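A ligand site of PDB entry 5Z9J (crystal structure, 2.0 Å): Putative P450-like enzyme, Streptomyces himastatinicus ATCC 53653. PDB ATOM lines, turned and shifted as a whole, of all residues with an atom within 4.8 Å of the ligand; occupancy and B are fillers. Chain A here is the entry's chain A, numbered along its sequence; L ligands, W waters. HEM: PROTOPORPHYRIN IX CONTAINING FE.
Water W3 lies within hydrogen-bond range of O1A of the ligand (2.7 Å), O of Ala 76 (3.1 Å), ND1 of His 345 (3.3 Å) and NH2 of Arg 289 (3.3 Å). Water W2 lies within hydrogen-bond range of the backbone carbonyl oxygen (O) of Gly 339 (2.6 Å) and the backbone carbonyl oxygen (O) of Ile 284 (2.8 Å).
O of Asn 237 lies close to NC of the ligand (3.3 Å). O of Ile 344 sits close to O2D of the ligand (3.5 Å). Merely in contact with the ligand: Phe 75 (3.4 Å), Ala 76 (3.3 Å), Arg 233 (3.9 Å), Leu 234 (3.7 Å), Gly 238 (3.3 Å), Thr 241 (3.5 Å), Thr 242 (3.7 Å), Leu 245 (3.6 Å), Ile 284 (3.9 Å), Val 287 (3.8 Å), Gly 339 (3.3 Å), Leu 340 (3.6 Å), Gly 341 (3.5 Å), Leu 348 (3.7 Å), Gly 349 (3.4 Å), Leu 352 (3.9 Å) and Ala 353 (3.7 Å). Within 4 Å of the ligand: Phe 75, Ala 76, His 83, Arg 87, Arg 233, Leu 234, Asn 237, Gly 238, Thr 241, Thr 242, Leu 245, Ile 284, Val 287, Arg 289, Gly 339, Leu 340, Gly 341, Ile 344, His 345, Cys 347, Leu 348, Gly 349, Leu 352 and Ala 353.
N of Gly 349 sits close to SG of Cys 347, 3.3 Å away. The backbone carbonyl oxygen (O) of Leu 340 lies within hydrogen-bond range of the backbone NH (N) of Cys 347. A ring nitrogen (NE2) of His 83 sits at hydrogen-bond distance from a ring nitrogen (ND1) of His 345 (3.4 Å). The guanidinium group of Arg 87 is in hydrogen-bond range of the backbone carbonyl oxygen of Ile 344 (3.2 Å). The backbone carbonyl oxygen of Phe 346 is in hydrogen-bond range of the guanidinium group of Arg 87, at 2.6 Å. The side-chain hydroxyl (OG1) of Thr 241 sits at hydrogen-bond distance from the backbone carbonyl oxygen (O) of Asn 237, 2.6 Å away. The guanidinium group (NH1) of Arg 233 sits at hydrogen-bond distance from the side-chain amide oxygen (OD1) of Asn 237 (3.0 Å). The side-chain hydroxyl of Thr 242 lies within hydrogen-bond range of the backbone carbonyl oxygen of Gly 238 (3.0 Å).
FE of the ligand is bound by SG of Cys 347, at 2.6 Å. O2D of the ligand sits at hydrogen-bond distance from NE2 of His 83 (2.7 Å). A ring nitrogen (ND1) of His 345 is in hydrogen-bond range of an oxygen (O1D) of the ligand. The guanidinium group (NH2) of Arg 289 lies within salt-bridge range of an oxygen (O2A) of the ligand (2.7 Å). The guanidinium group (NH1) of Arg 87 lies within salt-bridge range of an oxygen (O2D) of the ligand.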
ATOM      1  N   LEU A  48      37.125   2.295 -33.196  1.00  0.00           N
ATOM      2  CA  LEU A  48      35.939   3.089 -32.779  1.00  0.00           C
ATOM      3  C   LEU A  48      35.711   4.254 -33.766  1.00  0.00           C
ATOM      4  O   LEU A  48      34.571   4.659 -33.964  1.00  0.00           O
ATOM      5  CB  LEU A  48      36.124   3.617 -31.335  1.00  0.00           C
ATOM      6  CG  LEU A  48      36.207   2.559 -30.234  1.00  0.00           C
ATOM      7  CD1 LEU A  48      36.495   3.224 -28.882  1.00  0.00           C
ATOM      8  CD2 LEU A  48      34.891   1.738 -30.124  1.00  0.00           C
ATOM      9  N   PHE A  75      19.814   3.899 -31.124  1.00  0.00           N
ATOM     10  CA  PHE A  75      20.917   4.395 -31.936  1.00  0.00           C
ATOM     11  C   PHE A  75      22.280   3.915 -31.476  1.00  0.00           C
ATOM     12  O   PHE A  75      23.271   4.106 -32.172  1.00  0.00           O
ATOM     13  CB  PHE A  75      20.869   5.919 -32.006  1.00  0.00           C
ATOM     14  CG  PHE A  75      20.893   6.585 -30.689  1.00  0.00           C
ATOM     15  CD1 PHE A  75      19.713   6.861 -30.017  1.00  0.00           C
ATOM     16  CD2 PHE A  75      22.110   6.945 -30.108  1.00  0.00           C
ATOM     17  CE1 PHE A  75      19.732   7.494 -28.781  1.00  0.00           C
ATOM     18  CE2 PHE A  75      22.146   7.581 -28.877  1.00  0.00           C
ATOM     19  CZ  PHE A  75      20.942   7.861 -28.200  1.00  0.00           C
ATOM     20  N   ALA A  76      22.349   3.303 -30.301  1.00  0.00           N
ATOM     21  CA  ALA A  76      23.596   2.686 -29.843  1.00  0.00           C
ATOM     22  C   ALA A  76      23.965   1.500 -30.748  1.00  0.00           C
ATOM     23  O   ALA A  76      25.155   1.152 -30.894  1.00  0.00           O
ATOM     24  CB  ALA A  76      23.512   2.199 -28.370  1.00  0.00           C
ATOM     25  N   HIS A  83      22.285   6.718 -38.047  1.00  0.00           N
ATOM     26  CA  HIS A  83      22.679   7.045 -36.673  1.00  0.00           C
ATOM     27  C   HIS A  83      22.583   8.554 -36.327  1.00  0.00           C
ATOM     28  O   HIS A  83      22.033   8.931 -35.274  1.00  0.00           O
ATOM     29  CB  HIS A  83      24.108   6.578 -36.410  1.00  0.00           C
ATOM     30  CG  HIS A  83      24.660   6.971 -35.080  1.00  0.00           C
ATOM     31  ND1 HIS A  83      25.635   7.923 -34.910  1.00  0.00           N
ATOM     32  CD2 HIS A  83      24.364   6.512 -33.840  1.00  0.00           C
ATOM     33  CE1 HIS A  83      25.940   8.015 -33.634  1.00  0.00           C
ATOM     34  NE2 HIS A  83      25.173   7.178 -32.958  1.00  0.00           N
ATOM     35  N   ARG A  87      20.655  10.114 -33.034  1.00  0.00           N
ATOM     36  CA  ARG A  87      21.497  10.697 -32.015  1.00  0.00           C
ATOM     37  C   ARG A  87      21.276  12.212 -31.946  1.00  0.00           C
ATOM     38  O   ARG A  87      21.296  12.804 -30.850  1.00  0.00           O
ATOM     39  CB  ARG A  87      22.981  10.427 -32.277  1.00  0.00           C
ATOM     40  CG  ARG A  87      23.783  10.879 -31.063  1.00  0.00           C
ATOM     41  CD  ARG A  87      25.279  10.950 -31.225  1.00  0.00           C
ATOM     42  NE  ARG A  87      25.854  11.658 -30.083  1.00  0.00           N
ATOM     43  CZ  ARG A  87      26.601  11.105 -29.122  1.00  0.00           C
ATOM     44  NH1 ARG A  87      26.915   9.817 -29.152  1.00  0.00           N
ATOM     45  NH2 ARG A  87      27.081  11.890 -28.153  1.00  0.00           N
ATOM     46  N   PHE A  94      18.035  17.253 -25.331  1.00  0.00           N
ATOM     47  CA  PHE A  94      18.706  17.756 -24.121  1.00  0.00           C
ATOM     48  C   PHE A  94      18.886  19.242 -24.227  1.00  0.00           C
ATOM     49  O   PHE A  94      20.021  19.703 -24.355  1.00  0.00           O
ATOM     50  CB  PHE A  94      20.090  17.142 -23.940  1.00  0.00           C
ATOM     51  CG  PHE A  94      20.091  15.833 -23.210  1.00  0.00           C
ATOM     52  CD1 PHE A  94      19.561  14.701 -23.799  1.00  0.00           C
ATOM     53  CD2 PHE A  94      20.642  15.749 -21.959  1.00  0.00           C
ATOM     54  CE1 PHE A  94      19.575  13.492 -23.139  1.00  0.00           C
ATOM     55  CE2 PHE A  94      20.669  14.553 -21.290  1.00  0.00           C
ATOM     56  CZ  PHE A  94      20.123  13.405 -21.880  1.00  0.00           C
ATOM     57  N   ILE A 138      17.853  10.306 -14.161  1.00  0.00           N
ATOM     58  CA  ILE A 138      17.369   9.985 -15.485  1.00  0.00           C
ATOM     59  C   ILE A 138      15.843   9.870 -15.440  1.00  0.00           C
ATOM     60  O   ILE A 138      15.189  10.258 -16.363  1.00  0.00           O
ATOM     61  CB  ILE A 138      17.949   8.708 -16.048  1.00  0.00           C
ATOM     62  CG1 ILE A 138      19.506   8.856 -16.137  1.00  0.00           C
ATOM     63  CG2 ILE A 138      17.483   8.507 -17.455  1.00  0.00           C
ATOM     64  CD1 ILE A 138      20.167   7.575 -16.583  1.00  0.00           C
ATOM     65  N   ARG A 233      17.435   3.101 -23.709  1.00  0.00           N
ATOM     66  CA  ARG A 233      18.886   3.241 -23.928  1.00  0.00           C
ATOM     67  C   ARG A 233      19.470   4.279 -22.950  1.00  0.00           C
ATOM     68  O   ARG A 233      20.545   4.074 -22.418  1.00  0.00           O
ATOM     69  CB  ARG A 233      19.235   3.615 -25.385  1.00  0.00           C
ATOM     70  CG  ARG A 233      20.774   3.777 -25.666  1.00  0.00           C
ATOM     71  CD  ARG A 233      21.548   2.553 -25.163  1.00  0.00           C
ATOM     72  NE  ARG A 233      21.185   1.323 -25.867  1.00  0.00           N
ATOM     73  CZ  ARG A 233      21.433   0.073 -25.444  1.00  0.00           C
ATOM     74  NH1 ARG A 233      22.022  -0.157 -24.281  1.00  0.00           N
ATOM     75  NH2 ARG A 233      21.079  -0.959 -26.194  1.00  0.00           N
ATOM     76  N   LEU A 234      18.737   5.359 -22.673  1.00  0.00           N
ATOM     77  CA  LEU A 234      19.192   6.334 -21.696  1.00  0.00           C
ATOM     78  C   LEU A 234      19.270   5.698 -20.302  1.00  0.00           C
ATOM     79  O   LEU A 234      20.328   5.776 -19.636  1.00  0.00           O
ATOM     80  CB  LEU A 234      18.281   7.565 -21.693  1.00  0.00           C
ATOM     81  CG  LEU A 234      18.471   8.290 -23.028  1.00  0.00           C
ATOM     82  CD1 LEU A 234      17.535   9.398 -23.237  1.00  0.00           C
ATOM     83  CD2 LEU A 234      19.947   8.788 -23.147  1.00  0.00           C
ATOM     84  N   ASN A 237      22.018   2.898 -20.239  1.00  0.00           N
ATOM     85  CA  ASN A 237      23.393   3.408 -20.389  1.00  0.00           C
ATOM     86  C   ASN A 237      23.877   4.354 -19.324  1.00  0.00           C
ATOM     87  O   ASN A 237      25.109   4.563 -19.165  1.00  0.00           O
ATOM     88  CB  ASN A 237      23.589   4.053 -21.774  1.00  0.00           C
ATOM     89  CG  ASN A 237      23.915   2.997 -22.847  1.00  0.00           C
ATOM     90  OD1 ASN A 237      23.572   1.816 -22.705  1.00  0.00           O
ATOM     91  ND2 ASN A 237      24.585   3.423 -23.915  1.00  0.00           N
ATOM     92  N   GLY A 238      22.918   4.975 -18.668  1.00  0.00           N
ATOM     93  CA  GLY A 238      23.192   6.008 -17.699  1.00  0.00           C
ATOM     94  C   GLY A 238      23.037   5.633 -16.243  1.00  0.00           C
ATOM     95  O   GLY A 238      23.315   6.470 -15.402  1.00  0.00           O
ATOM     96  N   THR A 241      26.370   2.425 -14.939  1.00  0.00           N
ATOM     97  CA  THR A 241      27.659   2.965 -15.366  1.00  0.00           C
ATOM     98  C   THR A 241      28.077   4.089 -14.414  1.00  0.00           C
ATOM     99  O   THR A 241      29.228   4.166 -13.962  1.00  0.00           O
ATOM    100  CB  THR A 241      27.619   3.497 -16.820  1.00  0.00           C
ATOM    101  OG1 THR A 241      26.540   4.426 -17.000  1.00  0.00           O
ATOM    102  CG2 THR A 241      27.422   2.341 -17.764  1.00  0.00           C
ATOM    103  N   THR A 242      27.115   4.974 -14.143  1.00  0.00           N
ATOM    104  CA  THR A 242      27.303   6.121 -13.307  1.00  0.00           C
ATOM    105  C   THR A 242      27.413   5.734 -11.842  1.00  0.00           C
ATOM    106  O   THR A 242      28.252   6.305 -11.109  1.00  0.00           O
ATOM    107  CB  THR A 242      26.184   7.139 -13.468  1.00  0.00           C
ATOM    108  OG1 THR A 242      26.028   7.520 -14.839  1.00  0.00           O
ATOM    109  CG2 THR A 242      26.504   8.395 -12.679  1.00  0.00           C
ATOM    110  N   LEU A 245      31.022   4.545 -11.499  1.00  0.00           N
ATOM    111  CA  LEU A 245      31.975   5.608 -11.497  1.00  0.00           C
ATOM    112  C   LEU A 245      32.005   6.235 -10.091  1.00  0.00           C
ATOM    113  O   LEU A 245      33.054   6.552  -9.551  1.00  0.00           O
ATOM    114  CB  LEU A 245      31.605   6.655 -12.522  1.00  0.00           C
ATOM    115  CG  LEU A 245      32.530   7.875 -12.481  1.00  0.00           C
ATOM    116  CD1 LEU A 245      34.061   7.465 -12.655  1.00  0.00           C
ATOM    117  CD2 LEU A 245      32.136   8.896 -13.480  1.00  0.00           C
ATOM    118  N   MET A 278      37.676   6.594 -14.450  1.00  0.00           N
ATOM    119  CA  MET A 278      37.202   5.964 -15.685  1.00  0.00           C
ATOM    120  C   MET A 278      38.335   5.251 -16.427  1.00  0.00           C
ATOM    121  O   MET A 278      38.185   4.167 -16.945  1.00  0.00           O
ATOM    122  CB  MET A 278      36.518   7.014 -16.571  1.00  0.00           C
ATOM    123  CG  MET A 278      35.021   7.281 -16.068  1.00  0.00           C
ATOM    124  SD  MET A 278      34.160   8.325 -17.253  1.00  0.00           S
ATOM    125  CE  MET A 278      34.890   9.871 -16.899  1.00  0.00           C
ATOM    126  N   PRO A 283      33.849   1.692 -16.026  1.00  0.00           N
ATOM    127  CA  PRO A 283      32.506   1.101 -15.872  1.00  0.00           C
ATOM    128  C   PRO A 283      32.018   0.328 -17.087  1.00  0.00           C
ATOM    129  O   PRO A 283      31.408  -0.756 -16.978  1.00  0.00           O
ATOM    130  CB  PRO A 283      31.611   2.331 -15.605  1.00  0.00           C
ATOM    131  CG  PRO A 283      32.475   3.289 -14.943  1.00  0.00           C
ATOM    132  CD  PRO A 283      33.867   3.102 -15.587  1.00  0.00           C
ATOM    133  N   ILE A 284      32.260   0.888 -18.264  1.00  0.00           N
ATOM    134  CA  ILE A 284      32.124   0.119 -19.501  1.00  0.00           C
ATOM    135  C   ILE A 284      33.572  -0.201 -19.929  1.00  0.00           C
ATOM    136  O   ILE A 284      34.358   0.680 -20.300  1.00  0.00           O
ATOM    137  CB  ILE A 284      31.363   0.861 -20.597  1.00  0.00           C
ATOM    138  CG1 ILE A 284      29.916   1.167 -20.152  1.00  0.00           C
ATOM    139  CG2 ILE A 284      31.309   0.063 -21.863  1.00  0.00           C
ATOM    140  CD1 ILE A 284      29.036  -0.068 -19.947  1.00  0.00           C
ATOM    141  N   VAL A 287      33.389  -2.860 -25.539  1.00  0.00           N
ATOM    142  CA  VAL A 287      32.231  -2.708 -26.390  1.00  0.00           C
ATOM    143  C   VAL A 287      32.354  -3.597 -27.616  1.00  0.00           C
ATOM    144  O   VAL A 287      33.488  -3.881 -28.105  1.00  0.00           O
ATOM    145  CB  VAL A 287      32.003  -1.235 -26.844  1.00  0.00           C
ATOM    146  CG1 VAL A 287      31.820  -0.307 -25.613  1.00  0.00           C
ATOM    147  CG2 VAL A 287      33.122  -0.735 -27.683  1.00  0.00           C
ATOM    148  N   ARG A 289      31.627  -4.875 -31.567  1.00  0.00           N
ATOM    149  CA  ARG A 289      31.621  -4.366 -32.928  1.00  0.00           C
ATOM    150  C   ARG A 289      31.543  -5.557 -33.854  1.00  0.00           C
ATOM    151  O   ARG A 289      31.963  -6.655 -33.483  1.00  0.00           O
ATOM    152  CB  ARG A 289      32.879  -3.531 -33.175  1.00  0.00           C
ATOM    153  CG  ARG A 289      32.926  -2.197 -32.430  1.00  0.00           C
ATOM    154  CD  ARG A 289      31.827  -1.269 -32.865  1.00  0.00           C
ATOM    155  NE  ARG A 289      31.904   0.115 -32.405  1.00  0.00           N
ATOM    156  CZ  ARG A 289      31.399   0.566 -31.252  1.00  0.00           C
ATOM    157  NH1 ARG A 289      30.857  -0.272 -30.397  1.00  0.00           N
ATOM    158  NH2 ARG A 289      31.470   1.846 -30.945  1.00  0.00           N
ATOM    159  N   LEU A 338      39.426   5.836 -22.999  1.00  0.00           N
ATOM    160  CA  LEU A 338      38.343   5.389 -23.858  1.00  0.00           C
ATOM    161  C   LEU A 338      37.056   5.033 -23.080  1.00  0.00           C
ATOM    162  O   LEU A 338      36.113   4.409 -23.620  1.00  0.00           O
ATOM    163  CB  LEU A 338      38.801   4.177 -24.675  1.00  0.00           C
ATOM    164  CG  LEU A 338      39.934   4.449 -25.674  1.00  0.00           C
ATOM    165  CD1 LEU A 338      40.324   3.165 -26.428  1.00  0.00           C
ATOM    166  CD2 LEU A 338      39.487   5.545 -26.662  1.00  0.00           C
ATOM    167  N   GLY A 339      37.049   5.393 -21.799  1.00  0.00           N
ATOM    168  CA  GLY A 339      35.957   5.078 -20.904  1.00  0.00           C
ATOM    169  C   GLY A 339      34.586   5.523 -21.369  1.00  0.00           C
ATOM    170  O   GLY A 339      33.579   4.959 -20.942  1.00  0.00           O
ATOM    171  N   LEU A 340      34.585   6.560 -22.202  1.00  0.00           N
ATOM    172  CA  LEU A 340      33.386   7.169 -22.691  1.00  0.00           C
ATOM    173  C   LEU A 340      33.261   6.920 -24.189  1.00  0.00           C
ATOM    174  O   LEU A 340      32.411   7.506 -24.881  1.00  0.00           O
ATOM    175  CB  LEU A 340      33.403   8.682 -22.394  1.00  0.00           C
ATOM    176  CG  LEU A 340      33.059   9.034 -20.930  1.00  0.00           C
ATOM    177  CD1 LEU A 340      33.320  10.511 -20.607  1.00  0.00           C
ATOM    178  CD2 LEU A 340      31.673   8.624 -20.488  1.00  0.00           C
ATOM    179  N   GLY A 341      34.135   6.049 -24.687  1.00  0.00           N
ATOM    180  CA  GLY A 341      34.137   5.744 -26.083  1.00  0.00           C
ATOM    181  C   GLY A 341      34.945   6.742 -26.887  1.00  0.00           C
ATOM    182  O   GLY A 341      35.782   7.443 -26.354  1.00  0.00           O
ATOM    183  N   ILE A 344      31.561   8.514 -33.214  1.00  0.00           N
ATOM    184  CA  ILE A 344      30.162   8.894 -33.376  1.00  0.00           C
ATOM    185  C   ILE A 344      29.300   8.368 -32.256  1.00  0.00           C
ATOM    186  O   ILE A 344      28.235   8.929 -31.986  1.00  0.00           O
ATOM    187  CB  ILE A 344      29.595   8.473 -34.755  1.00  0.00           C
ATOM    188  CG1 ILE A 344      29.408   6.955 -34.922  1.00  0.00           C
ATOM    189  CG2 ILE A 344      30.493   9.066 -35.905  1.00  0.00           C
ATOM    190  CD1 ILE A 344      28.687   6.588 -36.211  1.00  0.00           C
ATOM    191  N   HIS A 345      29.742   7.287 -31.612  1.00  0.00           N
ATOM    192  CA  HIS A 345      28.993   6.706 -30.506  1.00  0.00           C
ATOM    193  C   HIS A 345      29.500   7.180 -29.140  1.00  0.00           C
ATOM    194  O   HIS A 345      29.077   6.665 -28.110  1.00  0.00           O
ATOM    195  CB  HIS A 345      29.008   5.179 -30.584  1.00  0.00           C
ATOM    196  CG  HIS A 345      28.233   4.626 -31.759  1.00  0.00           C
ATOM    197  ND1 HIS A 345      26.860   4.526 -31.768  1.00  0.00           N
ATOM    198  CD2 HIS A 345      28.658   4.166 -32.966  1.00  0.00           C
ATOM    199  CE1 HIS A 345      26.463   4.018 -32.930  1.00  0.00           C
ATOM    200  NE2 HIS A 345      27.529   3.798 -33.677  1.00  0.00           N
ATOM    201  N   PHE A 346      30.359   8.203 -29.152  1.00  0.00           N
ATOM    202  CA  PHE A 346      30.854   8.869 -27.930  1.00  0.00           C
ATOM    203  C   PHE A 346      29.745   9.215 -26.970  1.00  0.00           C
ATOM    204  O   PHE A 346      28.774   9.857 -27.379  1.00  0.00           O
ATOM    205  CB  PHE A 346      31.634  10.148 -28.322  1.00  0.00           C
ATOM    206  CG  PHE A 346      32.356  10.821 -27.198  1.00  0.00           C
ATOM    207  CD1 PHE A 346      33.356  10.146 -26.499  1.00  0.00           C
ATOM    208  CD2 PHE A 346      32.188  12.171 -26.971  1.00  0.00           C
ATOM    209  CE1 PHE A 346      34.064  10.778 -25.475  1.00  0.00           C
ATOM    210  CE2 PHE A 346      32.912  12.820 -25.969  1.00  0.00           C
ATOM    211  CZ  PHE A 346      33.847  12.119 -25.212  1.00  0.00           C
ATOM    212  N   CYS A 347      29.924   8.844 -25.688  1.00  0.00           N
ATOM    213  CA  CYS A 347      28.842   8.915 -24.688  1.00  0.00           C
ATOM    214  C   CYS A 347      28.025  10.186 -24.715  1.00  0.00           C
ATOM    215  O   CYS A 347      28.486  11.265 -24.395  1.00  0.00           O
ATOM    216  CB  CYS A 347      29.410   8.701 -23.279  1.00  0.00           C
ATOM    217  SG  CYS A 347      28.171   9.007 -22.020  1.00  0.00           S
ATOM    218  N   LEU A 348      26.753  10.038 -25.056  1.00  0.00           N
ATOM    219  CA  LEU A 348      25.810  11.150 -25.108  1.00  0.00           C
ATOM    220  C   LEU A 348      25.547  11.762 -23.743  1.00  0.00           C
ATOM    221  O   LEU A 348      25.252  12.938 -23.603  1.00  0.00           O
ATOM    222  CB  LEU A 348      24.467  10.645 -25.687  1.00  0.00           C
ATOM    223  CG  LEU A 348      23.297  11.635 -25.696  1.00  0.00           C
ATOM    224  CD1 LEU A 348      22.423  11.252 -26.864  1.00  0.00           C
ATOM    225  CD2 LEU A 348      22.462  11.625 -24.372  1.00  0.00           C
ATOM    226  N   GLY A 349      25.592  10.940 -22.723  1.00  0.00           N
ATOM    227  CA  GLY A 349      25.277  11.454 -21.390  1.00  0.00           C
ATOM    228  C   GLY A 349      26.528  11.890 -20.634  1.00  0.00           C
ATOM    229  O   GLY A 349      26.468  12.111 -19.458  1.00  0.00           O
ATOM    230  N   LEU A 352      26.084  15.007 -18.226  1.00  0.00           N
ATOM    231  CA  LEU A 352      25.313  14.633 -17.050  1.00  0.00           C
ATOM    232  C   LEU A 352      26.063  13.693 -16.100  1.00  0.00           C
ATOM    233  O   LEU A 352      25.944  13.808 -14.873  1.00  0.00           O
ATOM    234  CB  LEU A 352      23.982  13.978 -17.457  1.00  0.00           C
ATOM    235  CG  LEU A 352      23.188  13.335 -16.312  1.00  0.00           C
ATOM    236  CD1 LEU A 352      22.958  14.360 -15.195  1.00  0.00           C
ATOM    237  CD2 LEU A 352      21.785  12.880 -16.792  1.00  0.00           C
ATOM    238  N   ALA A 353      26.784  12.722 -16.667  1.00  0.00           N
ATOM    239  CA  ALA A 353      27.483  11.733 -15.843  1.00  0.00           C
ATOM    240  C   ALA A 353      28.591  12.380 -15.034  1.00  0.00           C
ATOM    241  O   ALA A 353      28.780  12.051 -13.867  1.00  0.00           O
ATOM    242  CB  ALA A 353      28.011  10.579 -16.703  1.00  0.00           C
ATOM    243  N   GLU A 356      26.965  14.737 -12.279  1.00  0.00           N
ATOM    244  CA  GLU A 356      26.462  13.908 -11.182  1.00  0.00           C
ATOM    245  C   GLU A 356      27.516  13.358 -10.293  1.00  0.00           C
ATOM    246  O   GLU A 356      27.410  13.356  -9.072  1.00  0.00           O
ATOM    247  CB  GLU A 356      25.736  12.672 -11.711  1.00  0.00           C
ATOM    248  CG  GLU A 356      24.463  12.875 -12.368  1.00  0.00           C
ATOM    249  CD  GLU A 356      23.824  11.553 -12.719  1.00  0.00           C
ATOM    250  OE1 GLU A 356      22.833  11.262 -12.038  1.00  0.00           O
ATOM    251  OE2 GLU A 356      24.277  10.814 -13.639  1.00  0.00           O
HETATM  252  CHA HEM L   1      27.581   5.852 -25.137  1.00  0.00           C
HETATM  253  CHB HEM L   1      30.139   4.965 -21.179  1.00  0.00           C
HETATM  254  CHC HEM L   1      26.933   7.561 -18.646  1.00  0.00           C
HETATM  255  CHD HEM L   1      23.926   7.616 -22.367  1.00  0.00           C
HETATM  256  C1A HEM L   1      28.602   5.385 -24.341  1.00  0.00           C
HETATM  257  C2A HEM L   1      29.785   4.631 -24.744  1.00  0.00           C
HETATM  258  C3A HEM L   1      30.508   4.397 -23.648  1.00  0.00           C
HETATM  259  C4A HEM L   1      29.789   4.986 -22.506  1.00  0.00           C
HETATM  260  CMA HEM L   1      31.840   3.630 -23.578  1.00  0.00           C
HETATM  261  CAA HEM L   1      30.159   4.193 -26.174  1.00  0.00           C
HETATM  262  CBA HEM L   1      29.370   2.948 -26.604  1.00  0.00           C
HETATM  263  CGA HEM L   1      29.924   2.321 -27.885  1.00  0.00           C
HETATM  264  O1A HEM L   1      29.489   1.212 -28.287  1.00  0.00           O
HETATM  265  O2A HEM L   1      30.786   2.910 -28.566  1.00  0.00           O
HETATM  266  C1B HEM L   1      29.526   5.652 -20.165  1.00  0.00           C
HETATM  267  C2B HEM L   1      30.084   5.834 -18.857  1.00  0.00           C
HETATM  268  C3B HEM L   1      29.195   6.556 -18.151  1.00  0.00           C
HETATM  269  C4B HEM L   1      28.045   6.819 -19.013  1.00  0.00           C
HETATM  270  CMB HEM L   1      31.453   5.274 -18.447  1.00  0.00           C
HETATM  271  CAB HEM L   1      29.251   7.051 -16.707  1.00  0.00           C
HETATM  272  CBB HEM L   1      30.295   6.867 -15.898  1.00  0.00           C
HETATM  273  C1C HEM L   1      25.832   7.843 -19.427  1.00  0.00           C
HETATM  274  C2C HEM L   1      24.627   8.618 -19.024  1.00  0.00           C
HETATM  275  C3C HEM L   1      23.811   8.625 -20.069  1.00  0.00           C
HETATM  276  C4C HEM L   1      24.443   7.857 -21.107  1.00  0.00           C
HETATM  277  CMC HEM L   1      24.470   9.296 -17.653  1.00  0.00           C
HETATM  278  CAC HEM L   1      22.405   9.230 -20.295  1.00  0.00           C
HETATM  279  CBC HEM L   1      21.761   9.973 -19.405  1.00  0.00           C
HETATM  280  C1D HEM L   1      24.619   7.114 -23.418  1.00  0.00           C
HETATM  281  C2D HEM L   1      24.052   6.908 -24.726  1.00  0.00           C
HETATM  282  C3D HEM L   1      25.191   6.390 -25.573  1.00  0.00           C
HETATM  283  C4D HEM L   1      26.337   6.311 -24.721  1.00  0.00           C
HETATM  284  CMD HEM L   1      22.593   7.159 -25.172  1.00  0.00           C
HETATM  285  CAD HEM L   1      25.086   5.960 -27.042  1.00  0.00           C
HETATM  286  CBD HEM L   1      25.440   7.109 -27.968  1.00  0.00           C
HETATM  287  CGD HEM L   1      25.521   6.569 -29.381  1.00  0.00           C
HETATM  288  O1D HEM L   1      25.566   5.336 -29.584  1.00  0.00           O
HETATM  289  O2D HEM L   1      25.573   7.389 -30.334  1.00  0.00           O
HETATM  290  NA  HEM L   1      28.663   5.568 -22.992  1.00  0.00           N
HETATM  291  NB  HEM L   1      28.268   6.249 -20.230  1.00  0.00           N
HETATM  292  NC  HEM L   1      25.631   7.397 -20.677  1.00  0.00           N
HETATM  293  ND  HEM L   1      25.981   6.784 -23.452  1.00  0.00           N
HETATM  294 FE   HEM L   1      27.152   6.634 -21.899  1.00  0.00          FE
HETATM  295  O   HOH W   1      27.629   2.279 -23.369  1.00  0.00           O
HETATM  296  O   HOH W   2      33.851   3.162 -19.088  1.00  0.00           O
HETATM  297  O   HOH W   3      28.185   1.757 -30.580  1.00  0.00           O
HETATM  298  O   HOH W   4      32.250   5.134 -29.082  1.00  0.00           O
HETATM  299  O   HOH W   5      26.642   3.860 -21.451  1.00  0.00           O
